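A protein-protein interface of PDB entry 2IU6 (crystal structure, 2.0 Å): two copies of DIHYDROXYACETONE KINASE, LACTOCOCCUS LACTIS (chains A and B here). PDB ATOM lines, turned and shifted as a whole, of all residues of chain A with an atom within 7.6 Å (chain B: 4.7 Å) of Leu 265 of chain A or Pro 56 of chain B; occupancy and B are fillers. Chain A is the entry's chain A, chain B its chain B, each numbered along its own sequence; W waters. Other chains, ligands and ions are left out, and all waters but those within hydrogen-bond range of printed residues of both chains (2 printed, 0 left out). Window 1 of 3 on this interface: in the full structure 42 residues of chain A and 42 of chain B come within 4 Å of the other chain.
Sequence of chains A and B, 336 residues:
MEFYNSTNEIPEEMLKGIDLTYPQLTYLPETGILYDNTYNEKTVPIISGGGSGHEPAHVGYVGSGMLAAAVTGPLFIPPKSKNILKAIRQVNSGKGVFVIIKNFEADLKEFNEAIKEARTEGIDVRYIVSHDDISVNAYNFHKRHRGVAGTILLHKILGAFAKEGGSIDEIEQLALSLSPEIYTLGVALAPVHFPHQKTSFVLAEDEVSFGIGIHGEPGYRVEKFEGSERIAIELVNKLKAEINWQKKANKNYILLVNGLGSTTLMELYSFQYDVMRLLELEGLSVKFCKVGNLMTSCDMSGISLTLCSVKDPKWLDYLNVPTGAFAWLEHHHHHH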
ATOM      1  N   VAL A 257     -13.042  -8.100   4.111  1.00  0.00           N
ATOM      2  CA  VAL A 257     -13.538  -9.354   4.648  1.00  0.00           C
ATOM      3  C   VAL A 257     -12.594  -9.792   5.770  1.00  0.00           C
ATOM      4  O   VAL A 257     -11.474 -10.231   5.510  1.00  0.00           O
ATOM      5  CB  VAL A 257     -13.579 -10.431   3.535  1.00  0.00           C
ATOM      6  CG1 VAL A 257     -14.123 -11.754   4.081  1.00  0.00           C
ATOM      7  CG2 VAL A 257     -14.418  -9.918   2.315  1.00  0.00           C
ATOM      8  N   GLY A 259     -11.546 -11.803   9.325  1.00  0.00           N
ATOM      9  CA  GLY A 259     -11.768 -12.945  10.203  1.00  0.00           C
ATOM     10  C   GLY A 259     -11.601 -12.518  11.643  1.00  0.00           C
ATOM     11  O   GLY A 259     -10.698 -11.771  11.966  1.00  0.00           O
ATOM     12  N   SER A 262     -10.540 -17.288  14.723  1.00  0.00           N
ATOM     13  CA  SER A 262     -10.237 -18.686  14.436  1.00  0.00           C
ATOM     14  C   SER A 262     -10.862 -19.160  13.117  1.00  0.00           C
ATOM     15  O   SER A 262     -10.741 -20.336  12.771  1.00  0.00           O
ATOM     16  CB  SER A 262     -10.601 -19.601  15.614  1.00  0.00           C
ATOM     17  OG  SER A 262     -12.004 -19.672  15.673  1.00  0.00           O
ATOM     18  N   THR A 263     -11.517 -18.267  12.379  1.00  0.00           N
ATOM     19  CA  THR A 263     -11.993 -18.608  11.037  1.00  0.00           C
ATOM     20  C   THR A 263     -10.805 -18.739  10.053  1.00  0.00           C
ATOM     21  O   THR A 263      -9.894 -17.892  10.066  1.00  0.00           O
ATOM     22  CB  THR A 263     -13.021 -17.535  10.617  1.00  0.00           C
ATOM     23  OG1 THR A 263     -14.101 -17.593  11.562  1.00  0.00           O
ATOM     24  CG2 THR A 263     -13.589 -17.763   9.231  1.00  0.00           C
ATOM     25  N   THR A 264     -10.798 -19.779   9.214  1.00  0.00           N
ATOM     26  CA  THR A 264      -9.622 -20.072   8.382  1.00  0.00           C
ATOM     27  C   THR A 264      -9.583 -19.228   7.106  1.00  0.00           C
ATOM     28  O   THR A 264     -10.581 -18.693   6.678  1.00  0.00           O
ATOM     29  CB  THR A 264      -9.620 -21.521   7.911  1.00  0.00           C
ATOM     30  OG1 THR A 264     -10.801 -21.762   7.119  1.00  0.00           O
ATOM     31  CG2 THR A 264      -9.653 -22.432   9.114  1.00  0.00           C
ATOM     32  N   LEU A 265      -8.412 -19.111   6.486  1.00  0.00           N
ATOM     33  CA  LEU A 265      -8.324 -18.451   5.183  1.00  0.00           C
ATOM     34  C   LEU A 265      -9.210 -19.116   4.146  1.00  0.00           C
ATOM     35  O   LEU A 265      -9.770 -18.444   3.273  1.00  0.00           O
ATOM     36  CB  LEU A 265      -6.867 -18.484   4.685  1.00  0.00           C
ATOM     37  CG  LEU A 265      -6.039 -17.200   4.749  1.00  0.00           C
ATOM     38  CD1 LEU A 265      -6.518 -15.931   5.500  1.00  0.00           C
ATOM     39  CD2 LEU A 265      -4.532 -17.408   4.719  1.00  0.00           C
ATOM     40  N   MET A 266      -9.358 -20.431   4.201  1.00  0.00           N
ATOM     41  CA  MET A 266     -10.247 -21.062   3.220  1.00  0.00           C
ATOM     42  C   MET A 266     -11.656 -20.476   3.395  1.00  0.00           C
ATOM     43  O   MET A 266     -12.336 -20.151   2.421  1.00  0.00           O
ATOM     44  CB  MET A 266     -10.270 -22.581   3.407  1.00  0.00           C
ATOM     45  CG  MET A 266     -11.093 -23.339   2.396  1.00  0.00           C
ATOM     46  SD  MET A 266     -12.862 -23.343   2.776  1.00  0.00           S
ATOM     47  CE  MET A 266     -12.874 -24.193   4.360  1.00  0.00           C
ATOM     48  N   GLU A 267     -12.121 -20.325   4.638  1.00  0.00           N
ATOM     49  CA  GLU A 267     -13.492 -19.807   4.828  1.00  0.00           C
ATOM     50  C   GLU A 267     -13.609 -18.334   4.447  1.00  0.00           C
ATOM     51  O   GLU A 267     -14.609 -17.894   3.873  1.00  0.00           O
ATOM     52  CB  GLU A 267     -13.864 -19.947   6.317  1.00  0.00           C
ATOM     53  CG  GLU A 267     -14.061 -21.394   6.735  1.00  0.00           C
ATOM     54  CD  GLU A 267     -14.079 -21.520   8.274  1.00  0.00           C
ATOM     55  OE1 GLU A 267     -13.008 -21.558   8.890  1.00  0.00           O
ATOM     56  OE2 GLU A 267     -15.168 -21.579   8.866  1.00  0.00           O
ATOM     57  N   LEU A 268     -12.587 -17.544   4.765  1.00  0.00           N
ATOM     58  CA  LEU A 268     -12.618 -16.109   4.491  1.00  0.00           C
ATOM     59  C   LEU A 268     -12.654 -15.818   3.012  1.00  0.00           C
ATOM     60  O   LEU A 268     -13.441 -14.987   2.606  1.00  0.00           O
ATOM     61  CB  LEU A 268     -11.366 -15.367   5.021  1.00  0.00           C
ATOM     62  CG  LEU A 268     -11.233 -15.286   6.546  1.00  0.00           C
ATOM     63  CD1 LEU A 268     -10.063 -14.370   6.921  1.00  0.00           C
ATOM     64  CD2 LEU A 268     -12.523 -14.751   7.199  1.00  0.00           C
ATOM     65  N   TYR A 269     -11.824 -16.471   2.198  1.00  0.00           N
ATOM     66  CA  TYR A 269     -11.828 -16.169   0.759  1.00  0.00           C
ATOM     67  C   TYR A 269     -13.082 -16.763   0.112  1.00  0.00           C
ATOM     68  O   TYR A 269     -13.616 -16.188  -0.828  1.00  0.00           O
ATOM     69  CB  TYR A 269     -10.551 -16.702   0.088  1.00  0.00           C
ATOM     70  CG  TYR A 269      -9.370 -15.791   0.325  1.00  0.00           C
ATOM     71  CD1 TYR A 269      -8.393 -16.117   1.278  1.00  0.00           C
ATOM     72  CD2 TYR A 269      -9.211 -14.604  -0.381  1.00  0.00           C
ATOM     73  CE1 TYR A 269      -7.298 -15.285   1.516  1.00  0.00           C
ATOM     74  CE2 TYR A 269      -8.091 -13.750  -0.147  1.00  0.00           C
ATOM     75  CZ  TYR A 269      -7.138 -14.103   0.811  1.00  0.00           C
ATOM     76  OH  TYR A 269      -6.030 -13.291   1.068  1.00  0.00           O
ATOM     77  N   SER A 270     -13.557 -17.908   0.613  1.00  0.00           N
ATOM     78  CA  SER A 270     -14.811 -18.485   0.135  1.00  0.00           C
ATOM     79  C   SER A 270     -15.924 -17.495   0.361  1.00  0.00           C
ATOM     80  O   SER A 270     -16.681 -17.215  -0.574  1.00  0.00           O
ATOM     81  CB  SER A 270     -15.118 -19.838   0.784  1.00  0.00           C
ATOM     82  OG  SER A 270     -14.099 -20.770   0.434  1.00  0.00           O
ATOM     83  N   PHE A 271     -16.020 -16.965   1.580  1.00  0.00           N
ATOM     84  CA  PHE A 271     -16.993 -15.909   1.895  1.00  0.00           C
ATOM     85  C   PHE A 271     -16.836 -14.653   1.036  1.00  0.00           C
ATOM     86  O   PHE A 271     -17.812 -14.100   0.551  1.00  0.00           O
ATOM     87  CB  PHE A 271     -16.933 -15.508   3.395  1.00  0.00           C
ATOM     88  CG  PHE A 271     -18.247 -14.921   3.947  1.00  0.00           C
ATOM     89  CD1 PHE A 271     -19.403 -15.683   4.001  1.00  0.00           C
ATOM     90  CD2 PHE A 271     -18.306 -13.598   4.413  1.00  0.00           C
ATOM     91  CE1 PHE A 271     -20.608 -15.156   4.507  1.00  0.00           C
ATOM     92  CE2 PHE A 271     -19.505 -13.055   4.920  1.00  0.00           C
ATOM     93  CZ  PHE A 271     -20.655 -13.833   4.967  1.00  0.00           C
ATOM     94  N   VAL A 291      -8.545  -8.980   2.597  1.00  0.00           N
ATOM     95  CA  VAL A 291      -9.111 -10.153   3.254  1.00  0.00           C
ATOM     96  C   VAL A 291      -8.022 -10.645   4.233  1.00  0.00           C
ATOM     97  O   VAL A 291      -6.835 -10.763   3.872  1.00  0.00           O
ATOM     98  CB  VAL A 291      -9.368 -11.301   2.206  1.00  0.00           C
ATOM     99  CG1 VAL A 291      -9.911 -12.606   2.890  1.00  0.00           C
ATOM    100  CG2 VAL A 291     -10.276 -10.805   1.018  1.00  0.00           C
ATOM    101  N   GLY A 292      -8.407 -10.933   5.477  1.00  0.00           N
ATOM    102  CA  GLY A 292      -7.483 -11.605   6.390  1.00  0.00           C
ATOM    103  C   GLY A 292      -7.957 -11.393   7.809  1.00  0.00           C
ATOM    104  O   GLY A 292      -9.090 -10.965   8.025  1.00  0.00           O
ATOM    105  N   ASN A 293      -7.087 -11.683   8.784  1.00  0.00           N
ATOM    106  CA  ASN A 293      -7.353 -11.337  10.181  1.00  0.00           C
ATOM    107  C   ASN A 293      -6.915  -9.882  10.390  1.00  0.00           C
ATOM    108  O   ASN A 293      -5.729  -9.615  10.641  1.00  0.00           O
ATOM    109  CB  ASN A 293      -6.601 -12.293  11.144  1.00  0.00           C
ATOM    110  CG  ASN A 293      -7.138 -13.746  11.120  1.00  0.00           C
ATOM    111  OD1 ASN A 293      -8.182 -14.051  10.525  1.00  0.00           O
ATOM    112  ND2 ASN A 293      -6.405 -14.656  11.769  1.00  0.00           N
ATOM    113  N   MET B  14     -12.935 -20.573  -2.648  1.00  0.00           N
ATOM    114  CA  MET B  14     -11.810 -19.938  -2.001  1.00  0.00           C
ATOM    115  C   MET B  14     -10.848 -19.478  -3.079  1.00  0.00           C
ATOM    116  O   MET B  14     -10.308 -18.366  -3.075  1.00  0.00           O
ATOM    117  CB  MET B  14     -11.059 -20.975  -1.189  1.00  0.00           C
ATOM    118  CG  MET B  14      -9.765 -20.337  -0.639  1.00  0.00           C
ATOM    119  SD  MET B  14      -8.669 -21.564   0.148  1.00  0.00           S
ATOM    120  CE  MET B  14      -7.792 -22.258  -1.272  1.00  0.00           C
ATOM    121  N   HIS B  54      -4.310 -26.094   4.618  1.00  0.00           N
ATOM    122  CA  HIS B  54      -3.004 -25.630   5.105  1.00  0.00           C
ATOM    123  C   HIS B  54      -2.737 -24.192   4.722  1.00  0.00           C
ATOM    124  O   HIS B  54      -1.644 -23.696   4.953  1.00  0.00           O
ATOM    125  CB  HIS B  54      -1.851 -26.461   4.540  1.00  0.00           C
ATOM    126  CG  HIS B  54      -1.947 -27.918   4.865  1.00  0.00           C
ATOM    127  ND1 HIS B  54      -1.881 -28.397   6.158  1.00  0.00           N
ATOM    128  CD2 HIS B  54      -2.097 -29.001   4.066  1.00  0.00           C
ATOM    129  CE1 HIS B  54      -1.998 -29.718   6.141  1.00  0.00           C
ATOM    130  NE2 HIS B  54      -2.120 -30.107   4.883  1.00  0.00           N
ATOM    131  N   GLU B  55      -3.730 -23.526   4.142  1.00  0.00           N
ATOM    132  CA  GLU B  55      -3.533 -22.170   3.624  1.00  0.00           C
ATOM    133  C   GLU B  55      -2.951 -21.232   4.707  1.00  0.00           C
ATOM    134  O   GLU B  55      -3.328 -21.308   5.854  1.00  0.00           O
ATOM    135  CB  GLU B  55      -4.934 -21.630   3.194  1.00  0.00           C
ATOM    136  CG  GLU B  55      -5.388 -22.315   1.885  1.00  0.00           C
ATOM    137  CD  GLU B  55      -6.208 -23.611   2.100  1.00  0.00           C
ATOM    138  OE1 GLU B  55      -6.469 -24.030   3.253  1.00  0.00           O
ATOM    139  OE2 GLU B  55      -6.617 -24.242   1.091  1.00  0.00           O
ATOM    140  N   PRO B  56      -2.053 -20.317   4.343  1.00  0.00           N
ATOM    141  CA  PRO B  56      -1.673 -19.982   2.957  1.00  0.00           C
ATOM    142  C   PRO B  56      -0.713 -20.900   2.226  1.00  0.00           C
ATOM    143  O   PRO B  56      -0.331 -20.552   1.112  1.00  0.00           O
ATOM    144  CB  PRO B  56      -1.034 -18.587   3.137  1.00  0.00           C
ATOM    145  CG  PRO B  56      -0.270 -18.731   4.487  1.00  0.00           C
ATOM    146  CD  PRO B  56      -1.355 -19.474   5.344  1.00  0.00           C
ATOM    147  N   ALA B  57      -0.287 -22.050   2.772  1.00  0.00           N
ATOM    148  CA  ALA B  57       0.464 -23.019   1.894  1.00  0.00           C
ATOM    149  C   ALA B  57      -0.523 -23.784   0.982  1.00  0.00           C
ATOM    150  O   ALA B  57      -1.371 -24.526   1.512  1.00  0.00           O
ATOM    151  CB  ALA B  57       1.239 -24.022   2.778  1.00  0.00           C
ATOM    152  N   HIS B  58      -0.456 -23.629  -0.349  1.00  0.00           N
ATOM    153  CA  HIS B  58       0.679 -22.923  -1.008  1.00  0.00           C
ATOM    154  C   HIS B  58       0.182 -21.704  -1.802  1.00  0.00           C
ATOM    155  O   HIS B  58       0.984 -21.021  -2.451  1.00  0.00           O
ATOM    156  CB  HIS B  58       1.409 -23.949  -1.913  1.00  0.00           C
ATOM    157  CG  HIS B  58       1.875 -25.151  -1.148  1.00  0.00           C
ATOM    158  ND1 HIS B  58       3.012 -25.131  -0.362  1.00  0.00           N
ATOM    159  CD2 HIS B  58       1.356 -26.398  -1.030  1.00  0.00           C
ATOM    160  CE1 HIS B  58       3.171 -26.318   0.204  1.00  0.00           C
ATOM    161  NE2 HIS B  58       2.181 -27.106  -0.184  1.00  0.00           N
ATOM    162  N   VAL B  59      -1.127 -21.436  -1.763  1.00  0.00           N
ATOM    163  CA  VAL B  59      -1.702 -20.339  -2.556  1.00  0.00           C
ATOM    164  C   VAL B  59      -1.090 -18.960  -2.207  1.00  0.00           C
ATOM    165  O   VAL B  59      -1.058 -18.059  -3.037  1.00  0.00           O
ATOM    166  CB  VAL B  59      -3.240 -20.265  -2.462  1.00  0.00           C
ATOM    167  CG1 VAL B  59      -3.879 -21.563  -3.113  1.00  0.00           C
ATOM    168  CG2 VAL B  59      -3.732 -20.165  -0.982  1.00  0.00           C
ATOM    169  N   GLY B  60      -0.627 -18.791  -0.972  1.00  0.00           N
ATOM    170  CA  GLY B  60      -0.142 -17.481  -0.550  1.00  0.00           C
ATOM    171  C   GLY B  60       1.319 -17.278  -0.902  1.00  0.00           C
ATOM    172  O   GLY B  60       1.906 -16.209  -0.576  1.00  0.00           O
ATOM    173  N   TYR B  61       1.912 -18.285  -1.564  1.00  0.00           N
ATOM    174  CA  TYR B  61       3.331 -18.251  -1.990  1.00  0.00           C
ATOM    175  C   TYR B  61       3.478 -18.273  -3.505  1.00  0.00           C
ATOM    176  O   TYR B  61       4.566 -18.496  -4.026  1.00  0.00           O
ATOM    177  CB  TYR B  61       4.114 -19.415  -1.328  1.00  0.00           C
ATOM    178  CG  TYR B  61       3.929 -19.340   0.180  1.00  0.00           C
ATOM    179  CD1 TYR B  61       4.462 -18.271   0.903  1.00  0.00           C
ATOM    180  CD2 TYR B  61       3.205 -20.316   0.876  1.00  0.00           C
ATOM    181  CE1 TYR B  61       4.306 -18.162   2.293  1.00  0.00           C
ATOM    182  CE2 TYR B  61       3.044 -20.205   2.292  1.00  0.00           C
ATOM    183  CZ  TYR B  61       3.588 -19.149   2.971  1.00  0.00           C
ATOM    184  OH  TYR B  61       3.419 -19.051   4.345  1.00  0.00           O
ATOM    185  N   ASN B 293       0.555 -17.060  10.510  1.00  0.00           N
ATOM    186  CA  ASN B 293      -0.031 -18.333  10.089  1.00  0.00           C
ATOM    187  C   ASN B 293       0.617 -18.655   8.748  1.00  0.00           C
ATOM    188  O   ASN B 293       0.152 -18.154   7.740  1.00  0.00           O
ATOM    189  CB  ASN B 293      -1.559 -18.212   9.973  1.00  0.00           C
ATOM    190  CG  ASN B 293      -2.239 -18.072  11.318  1.00  0.00           C
ATOM    191  OD1 ASN B 293      -1.610 -18.197  12.377  1.00  0.00           O
ATOM    192  ND2 ASN B 293      -3.556 -17.796  11.283  1.00  0.00           N
ATOM    193  N   LEU B 294       1.688 -19.461   8.726  1.00  0.00           N
ATOM    194  CA  LEU B 294       2.468 -19.654   7.486  1.00  0.00           C
ATOM    195  C   LEU B 294       2.089 -20.949   6.792  1.00  0.00           C
ATOM    196  O   LEU B 294       2.099 -21.033   5.565  1.00  0.00           O
ATOM    197  CB  LEU B 294       3.986 -19.612   7.746  1.00  0.00           C
ATOM    198  CG  LEU B 294       4.504 -18.531   8.714  1.00  0.00           C
ATOM    199  CD1 LEU B 294       6.071 -18.657   8.876  1.00  0.00           C
ATOM    200  CD2 LEU B 294       4.116 -17.114   8.206  1.00  0.00           C
ATOM    201  N   MET B 295       1.743 -21.955   7.601  1.00  0.00           N
ATOM    202  CA  MET B 295       1.169 -23.204   7.073  1.00  0.00           C
ATOM    203  C   MET B 295       0.296 -23.793   8.158  1.00  0.00           C
ATOM    204  O   MET B 295       0.809 -24.171   9.217  1.00  0.00           O
ATOM    205  CB  MET B 295       2.273 -24.204   6.693  1.00  0.00           C
ATOM    206  CG  MET B 295       1.679 -25.582   6.329  1.00  0.00           C
ATOM    207  SD  MET B 295       2.885 -26.703   5.563  1.00  0.00           S
ATOM    208  CE  MET B 295       1.905 -28.214   5.491  1.00  0.00           C
ATOM    209  N   PHE B 326       1.030 -13.300  -1.718  1.00  0.00           N
ATOM    210  CA  PHE B 326       0.319 -12.553  -0.702  1.00  0.00           C
ATOM    211  C   PHE B 326       0.758 -12.834   0.742  1.00  0.00           C
ATOM    212  O   PHE B 326       0.571 -12.019   1.624  1.00  0.00           O
ATOM    213  CB  PHE B 326      -1.204 -12.561  -0.924  1.00  0.00           C
ATOM    214  CG  PHE B 326      -1.941 -13.833  -0.530  1.00  0.00           C
ATOM    215  CD1 PHE B 326      -2.120 -14.170   0.814  1.00  0.00           C
ATOM    216  CD2 PHE B 326      -2.478 -14.672  -1.500  1.00  0.00           C
ATOM    217  CE1 PHE B 326      -2.820 -15.339   1.192  1.00  0.00           C
ATOM    218  CE2 PHE B 326      -3.177 -15.840  -1.132  1.00  0.00           C
ATOM    219  CZ  PHE B 326      -3.349 -16.163   0.210  1.00  0.00           C
ATOM    220  N   ALA B 327       1.345 -14.000   0.999  1.00  0.00           N
ATOM    221  CA  ALA B 327       1.715 -14.312   2.385  1.00  0.00           C
ATOM    222  C   ALA B 327       3.212 -14.055   2.575  1.00  0.00           C
ATOM    223  O   ALA B 327       3.771 -14.367   3.614  1.00  0.00           O
ATOM    224  CB  ALA B 327       1.389 -15.754   2.738  1.00  0.00           C
HETATM  225  O   HOH W   1     -14.119 -23.120  -1.233  1.00  0.00           O
HETATM  226  O   HOH W   2      -7.602 -22.844   5.432  1.00  0.00           O
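N of Met 14 of chain B lies within hydrogen-bond range of OG of Ser 270 of chain A (3.3 Å).
The backbone NH (N) of Phe 326 of chain B sits at hydrogen-bond distance from the backbone carbonyl oxygen (O) of Gly 60 of chain B. OG of Ser 270 of chain A sits at hydrogen-bond distance from O of Met 266 of chain A (2.7 Å).
Among the printed residues, merely in contact across the chains: Met 266 of chain A with Met 14 of chain B (3.5 Å), Tyr 269 of chain A with Met 14 of chain B (3.6 Å), Tyr 269 of chain A with Phe 326 of chain B (3.8 Å), Leu 265 of chain A with Pro 56 of chain B (3.8 Å) and Leu 265 of chain A with Glu 55 of chain B (3.98 Å).
Printed residues of chain B within 4 Å of Leu 265 of chain A: Glu 55 and Pro 56. Of chain A, only Leu 265 (3.8 Å) comes within 4 Å of Pro 56 of chain B. Printed residues of chain B within 4 Å of Tyr 269 of chain A: Met 14 and Phe 326. Printed residues of chain B within 4 Å of Ser 270 of chain A: Met 14 (3.3 Å). Of the printed residues of chain A, Phe 326 of chain B touches Tyr 269. Printed residues of chain A within 4 Å of Glu 55 of chain B: Leu 265. Thr 263 of chain A touches none of the printed residues of chain B. The nearest printed residue of chain B that does not touch Leu 265 of chain A is Met 14 of chain B (4.3 Å). The nearest residue of chain A that does not touch Pro 56 of chain B is Tyr 269 of chain A (7.3 Å). The nearest printed residue of chain A that does not touch Met 14 of chain B is Leu 265 of chain A (4.3 Å).
Of the 14 printed residues of chain B, 4 touch a printed residue of chain A. Hydrophobic or aromatic side chains of chain A within 4 Å of the printed part of chain B: Leu 265, Met 266 and Tyr 269. Among the printed residues, 6 pairs touch across the chains.
1 position is printed for both chains. Of the 6 pairs that touch across the chains among the printed residues, none has its exchanged pair printed and touching as well.
Water W2 lies within hydrogen-bond range of the side-chain carboxylate of Glu 55 of chain B (2.7 Å) and the backbone NH of Met 266 of chain A (3.2 Å). Water W1 bridges the side-chain hydroxyl of Ser 270 of chain A and the backbone NH of Met 14 of chain B.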
